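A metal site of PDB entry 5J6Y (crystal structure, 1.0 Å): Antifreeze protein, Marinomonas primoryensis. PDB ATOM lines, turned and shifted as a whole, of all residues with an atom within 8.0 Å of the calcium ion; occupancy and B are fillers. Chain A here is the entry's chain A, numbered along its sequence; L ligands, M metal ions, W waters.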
ATOM      1  N   THR A  21       1.105   8.202   4.235  1.00  0.00           N
ATOM      2  CA  THR A  21       0.497   8.000   2.932  1.00  0.00           C
ATOM      3  C   THR A  21      -0.676   8.949   2.764  1.00  0.00           C
ATOM      4  O   THR A  21      -1.237   9.441   3.739  1.00  0.00           O
ATOM      5  CB  THR A  21       0.033   6.522   2.774  1.00  0.00           C
ATOM      6  OG1 THR A  21      -0.504   6.324   1.474  1.00  0.00           O
ATOM      7  CG2 THR A  21      -1.037   6.149   3.763  1.00  0.00           C
ATOM      8  N   ASN A  22      -1.056   9.206   1.511  1.00  0.00           N
ATOM      9  CA  ASN A  22      -2.258   9.976   1.227  1.00  0.00           C
ATOM     10  C   ASN A  22      -3.405   9.078   0.726  1.00  0.00           C
ATOM     11  O   ASN A  22      -4.444   9.578   0.266  1.00  0.00           O
ATOM     12  CB  ASN A  22      -1.961  11.102   0.255  1.00  0.00           C
ATOM     13  CG  ASN A  22      -0.911  12.033   0.819  1.00  0.00           C
ATOM     14  OD1 ASN A  22      -0.967  12.371   2.020  1.00  0.00           O
ATOM     15  ND2 ASN A  22       0.028  12.446   0.007  1.00  0.00           N
ATOM     16  N   SER A  23      -3.218   7.767   0.862  1.00  0.00           N
ATOM     17  CA  SER A  23      -4.276   6.788   0.666  1.00  0.00           C
ATOM     18  C   SER A  23      -4.904   6.449   2.012  1.00  0.00           C
ATOM     19  O   SER A  23      -4.334   6.745   3.071  1.00  0.00           O
ATOM     20  CB  SER A  23      -3.708   5.522   0.014  1.00  0.00           C
ATOM     21  OG  SER A  23      -2.843   4.837   0.909  1.00  0.00           O
ATOM     22  N   GLN A  24      -6.087   5.838   1.975  1.00  0.00           N
ATOM     23  CA  GLN A  24      -6.775   5.479   3.199  1.00  0.00           C
ATOM     24  C   GLN A  24      -6.245   4.176   3.794  1.00  0.00           C
ATOM     25  O   GLN A  24      -6.123   3.174   3.101  1.00  0.00           O
ATOM     26  CB  GLN A  24      -8.290   5.353   2.943  1.00  0.00           C
ATOM     27  CG  GLN A  24      -9.060   4.677   4.056  1.00  0.00           C
ATOM     28  CD  GLN A  24      -9.211   5.526   5.304  1.00  0.00           C
ATOM     29  OE1 GLN A  24      -8.539   6.537   5.464  1.00  0.00           O
ATOM     30  NE2 GLN A  24     -10.096   5.102   6.197  1.00  0.00           N
ATOM     31  N   LEU A  25      -5.948   4.208   5.083  1.00  0.00           N
ATOM     32  CA  LEU A  25      -5.620   2.998   5.830  1.00  0.00           C
ATOM     33  C   LEU A  25      -6.876   2.498   6.545  1.00  0.00           C
ATOM     34  O   LEU A  25      -7.387   3.164   7.433  1.00  0.00           O
ATOM     35  CB  LEU A  25      -4.511   3.282   6.846  1.00  0.00           C
ATOM     36  CG  LEU A  25      -3.170   3.720   6.233  1.00  0.00           C
ATOM     37  CD1 LEU A  25      -2.241   4.136   7.351  1.00  0.00           C
ATOM     38  CD2 LEU A  25      -2.558   2.644   5.366  1.00  0.00           C
ATOM     39  N   ASN A  26      -7.375   1.332   6.126  1.00  0.00           N
ATOM     40  CA  ASN A  26      -8.587   0.761   6.714  1.00  0.00           C
ATOM     41  C   ASN A  26      -8.348  -0.406   7.656  1.00  0.00           C
ATOM     42  O   ASN A  26      -9.244  -0.784   8.412  1.00  0.00           O
ATOM     43  CB  ASN A  26      -9.574   0.290   5.628  1.00  0.00           C
ATOM     44  CG  ASN A  26     -10.318   1.427   4.985  1.00  0.00           C
ATOM     45  OD1 ASN A  26     -10.855   2.301   5.675  1.00  0.00           O
ATOM     46  ND2 ASN A  26     -10.402   1.417   3.659  1.00  0.00           N
ATOM     47  N   ASP A  57      -4.804  14.499  13.070  1.00  0.00           N
ATOM     48  CA  ASP A  57      -4.073  13.596  12.152  1.00  0.00           C
ATOM     49  C   ASP A  57      -2.613  13.398  12.557  1.00  0.00           C
ATOM     50  O   ASP A  57      -1.832  14.354  12.594  1.00  0.00           O
ATOM     51  CB  ASP A  57      -4.072  14.074  10.699  1.00  0.00           C
ATOM     52  CG  ASP A  57      -5.423  14.431  10.188  1.00  0.00           C
ATOM     53  OD1 ASP A  57      -6.402  13.740  10.446  1.00  0.00           O
ATOM     54  OD2 ASP A  57      -5.516  15.419   9.420  1.00  0.00           O
ATOM     55  N   ASN A  82       1.240  14.024   5.491  1.00  0.00           N
ATOM     56  CA  ASN A  82       0.412  13.031   4.816  1.00  0.00           C
ATOM     57  C   ASN A  82      -0.955  13.016   5.502  1.00  0.00           C
ATOM     58  O   ASN A  82      -1.114  13.598   6.578  1.00  0.00           O
ATOM     59  CB  ASN A  82       1.018  11.630   4.907  1.00  0.00           C
ATOM     60  CG  ASN A  82       2.111  11.401   3.873  1.00  0.00           C
ATOM     61  OD1 ASN A  82       1.832  11.340   2.663  1.00  0.00           O
ATOM     62  ND2 ASN A  82       3.318  11.215   4.325  1.00  0.00           N
ATOM     63  N   THR A  83      -1.935  12.369   4.892  1.00  0.00           N
ATOM     64  CA  THR A  83      -3.254  12.271   5.537  1.00  0.00           C
ATOM     65  C   THR A  83      -3.300  11.154   6.569  1.00  0.00           C
ATOM     66  O   THR A  83      -3.990  11.294   7.574  1.00  0.00           O
ATOM     67  CB  THR A  83      -4.388  12.095   4.503  1.00  0.00           C
ATOM     68  OG1 THR A  83      -4.260  10.833   3.835  1.00  0.00           O
ATOM     69  CG2 THR A  83      -4.342  13.175   3.443  1.00  0.00           C
ATOM     70  N   ASP A  84      -2.604  10.057   6.302  1.00  0.00           N
ATOM     71  CA  ASP A  84      -2.674   8.828   7.087  1.00  0.00           C
ATOM     72  C   ASP A  84      -1.252   8.394   7.420  1.00  0.00           C
ATOM     73  O   ASP A  84      -0.320   8.703   6.669  1.00  0.00           O
ATOM     74  CB  ASP A  84      -3.338   7.713   6.262  1.00  0.00           C
ATOM     75  CG  ASP A  84      -4.834   7.931   5.997  1.00  0.00           C
ATOM     76  OD1 ASP A  84      -5.208   9.032   5.535  1.00  0.00           O
ATOM     77  OD2 ASP A  84      -5.643   6.994   6.236  1.00  0.00           O
ATOM     78  N   GLY A  85      -1.046   7.682   8.514  1.00  0.00           N
ATOM     79  CA  GLY A  85       0.293   7.211   8.797  1.00  0.00           C
ATOM     80  C   GLY A  85       0.302   6.217   9.929  1.00  0.00           C
ATOM     81  O   GLY A  85      -0.706   6.048  10.625  1.00  0.00           O
ATOM     82  N   ASP A 108      -5.883   4.337  15.607  1.00  0.00           N
ATOM     83  CA  ASP A 108      -6.887   3.426  15.092  1.00  0.00           C
ATOM     84  C   ASP A 108      -6.540   1.983  15.499  1.00  0.00           C
ATOM     85  O   ASP A 108      -6.551   1.685  16.706  1.00  0.00           O
ATOM     86  CB  ASP A 108      -7.042   3.648  13.584  1.00  0.00           C
ATOM     87  CG  ASP A 108      -7.844   4.894  13.296  1.00  0.00           C
ATOM     88  OD1 ASP A 108      -9.097   4.793  13.397  1.00  0.00           O
ATOM     89  OD2 ASP A 108      -7.257   5.991  13.047  1.00  0.00           O
ATOM     90  N   ASN A 125     -10.442   0.428  11.810  1.00  0.00           N
ATOM     91  CA  ASN A 125     -10.356   1.749  12.384  1.00  0.00           C
ATOM     92  C   ASN A 125     -11.288   1.874  13.563  1.00  0.00           C
ATOM     93  O   ASN A 125     -12.263   1.125  13.685  1.00  0.00           O
ATOM     94  CB  ASN A 125     -10.667   2.787  11.304  1.00  0.00           C
ATOM     95  CG  ASN A 125      -9.550   2.892  10.289  1.00  0.00           C
ATOM     96  OD1 ASN A 125      -8.374   2.745  10.655  1.00  0.00           O
ATOM     97  ND2 ASN A 125      -9.879   3.182   9.046  1.00  0.00           N
ATOM     98  N   TRP A 151      -1.660   2.251  13.305  1.00  0.00           N
ATOM     99  CA  TRP A 151      -1.824   3.351  12.363  1.00  0.00           C
ATOM    100  C   TRP A 151      -2.957   4.266  12.782  1.00  0.00           C
ATOM    101  O   TRP A 151      -3.795   3.925  13.627  1.00  0.00           O
ATOM    102  CB  TRP A 151      -2.072   2.824  10.935  1.00  0.00           C
ATOM    103  CG  TRP A 151      -3.468   2.301  10.750  1.00  0.00           C
ATOM    104  CD1 TRP A 151      -4.561   2.993  10.322  1.00  0.00           C
ATOM    105  CD2 TRP A 151      -3.936   0.982  11.059  1.00  0.00           C
ATOM    106  NE1 TRP A 151      -5.670   2.194  10.332  1.00  0.00           N
ATOM    107  CE2 TRP A 151      -5.315   0.956  10.809  1.00  0.00           C
ATOM    108  CE3 TRP A 151      -3.327  -0.178  11.553  1.00  0.00           C
ATOM    109  CZ2 TRP A 151      -6.098  -0.185  10.987  1.00  0.00           C
ATOM    110  CZ3 TRP A 151      -4.119  -1.302  11.762  1.00  0.00           C
ATOM    111  CH2 TRP A 151      -5.485  -1.289  11.484  1.00  0.00           C
ATOM    112  N   ASP A 152      -2.956   5.426  12.132  1.00  0.00           N
ATOM    113  CA  ASP A 152      -4.001   6.436  12.205  1.00  0.00           C
ATOM    114  C   ASP A 152      -4.535   6.707  10.805  1.00  0.00           C
ATOM    115  O   ASP A 152      -3.768   7.073   9.902  1.00  0.00           O
ATOM    116  CB  ASP A 152      -3.438   7.741  12.779  1.00  0.00           C
ATOM    117  CG  ASP A 152      -4.452   8.861  12.766  1.00  0.00           C
ATOM    118  OD1 ASP A 152      -5.656   8.566  13.010  1.00  0.00           O
ATOM    119  OD2 ASP A 152      -4.077  10.021  12.477  1.00  0.00           O
ATOM    120  N   GLN A 153      -5.834   6.503  10.605  1.00  0.00           N
ATOM    121  CA  GLN A 153      -6.492   6.836   9.340  1.00  0.00           C
ATOM    122  C   GLN A 153      -6.843   8.322   9.262  1.00  0.00           C
ATOM    123  O   GLN A 153      -7.313   8.795   8.209  1.00  0.00           O
ATOM    124  CB  GLN A 153      -7.770   6.005   9.180  1.00  0.00           C
ATOM    125  CG  GLN A 153      -8.894   6.355  10.109  1.00  0.00           C
ATOM    126  CD  GLN A 153      -9.865   7.337   9.483  1.00  0.00           C
ATOM    127  OE1 GLN A 153     -10.396   7.127   8.382  1.00  0.00           O
ATOM    128  NE2 GLN A 153     -10.078   8.421  10.158  1.00  0.00           N
ATOM    129  N   GLY A 154      -6.658   9.050  10.358  1.00  0.00           N
ATOM    130  CA  GLY A 154      -7.063  10.433  10.441  1.00  0.00           C
ATOM    131  C   GLY A 154      -7.763  10.710  11.757  1.00  0.00           C
ATOM    132  O   GLY A 154      -8.245   9.816  12.428  1.00  0.00           O
ATOM    133  N   GLY A 155      -7.751  11.986  12.133  1.00  0.00           N
ATOM    134  CA  GLY A 155      -8.440  12.443  13.341  1.00  0.00           C
ATOM    135  C   GLY A 155      -7.592  12.318  14.575  1.00  0.00           C
ATOM    136  O   GLY A 155      -6.461  12.815  14.619  1.00  0.00           O
HETATM  137  C1  LIG L   1     -13.301   9.107  14.687  1.00  0.00           C
HETATM  138  C2  LIG L   1     -12.001   9.421  15.413  1.00  0.00           C
HETATM  139  C3  LIG L   1     -10.841   9.005  14.560  1.00  0.00           C
HETATM  140  C4  LIG L   1     -10.950   7.555  14.172  1.00  0.00           C
HETATM  141  C5  LIG L   1     -12.281   7.339  13.409  1.00  0.00           C
HETATM  142  C6  LIG L   1     -12.480   5.866  13.043  1.00  0.00           C
HETATM  143  O1  LIG L   1     -13.362   9.900  13.568  1.00  0.00           O
HETATM  144  O2  LIG L   1     -11.922  10.807  15.712  1.00  0.00           O
HETATM  145  O3  LIG L   1      -9.569   9.231  15.218  1.00  0.00           O
HETATM  146  O4  LIG L   1      -9.860   7.266  13.265  1.00  0.00           O
HETATM  147  O5  LIG L   1     -13.359   7.747  14.288  1.00  0.00           O
HETATM  148  O6  LIG L   1     -13.705   5.792  12.253  1.00  0.00           O
HETATM  149 CA    CA M   1      -7.564   8.581   5.908  1.00  0.00          CA
HETATM  150  O   HOH W   1      -7.780  10.971   5.864  1.00  0.00           O
HETATM  151  O   HOH W   2      -7.917   8.784   3.582  1.00  0.00           O
HETATM  152  O   HOH W   3      -9.903   8.989   6.443  1.00  0.00           O
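The side-chain amide nitrogen of Gln 153 sits close to an oxygen (O4) of the ligand, 3.3 Å away.
NE2 of Gln 24 lies within hydrogen-bond range of OD1 of Asn 26 (2.9 Å).
The side-chain amide nitrogen (NE2) of Gln 24 lies close to the side-chain amide nitrogen (ND2) of Asn 125.
OD2 of Asp 84 sits close to N of Leu 25, at 3.0 Å.
The backbone NH of Thr 21 sits at hydrogen-bond distance from the backbone carbonyl oxygen of Asp 84, at 2.9 Å.
OD1 of Asp 84 lies close to OG1 of Thr 83 (2.7 Å).
The backbone NH of Gln 153 lies close to the side-chain carboxylate of Asp 108 (2.9 Å).
Within 4 Å of the calcium ion: Gln 24, Asp 84 and Gln 153.
The nearest printed residue that does not touch the calcium ion is Thr 83 (4.5 Å).
OE1 of Gln 24 is bound to the calcium ion, 2.3 Å away.
The backbone carbonyl oxygen (O) of Gln 153 is bound to the calcium ion, 2.3 Å away.
The calcium ion is bound by water W2 (2.4 Å).
Water W1 is bound to the calcium ion (2.4 Å).
The calcium ion is bound by the side-chain carboxylate (OD1) of Asp 84 (2.4 Å).
The calcium ion is bound by water W3 (2.4 Å).
The calcium ion is bound by OD2 of Asp 84 (2.5 Å).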
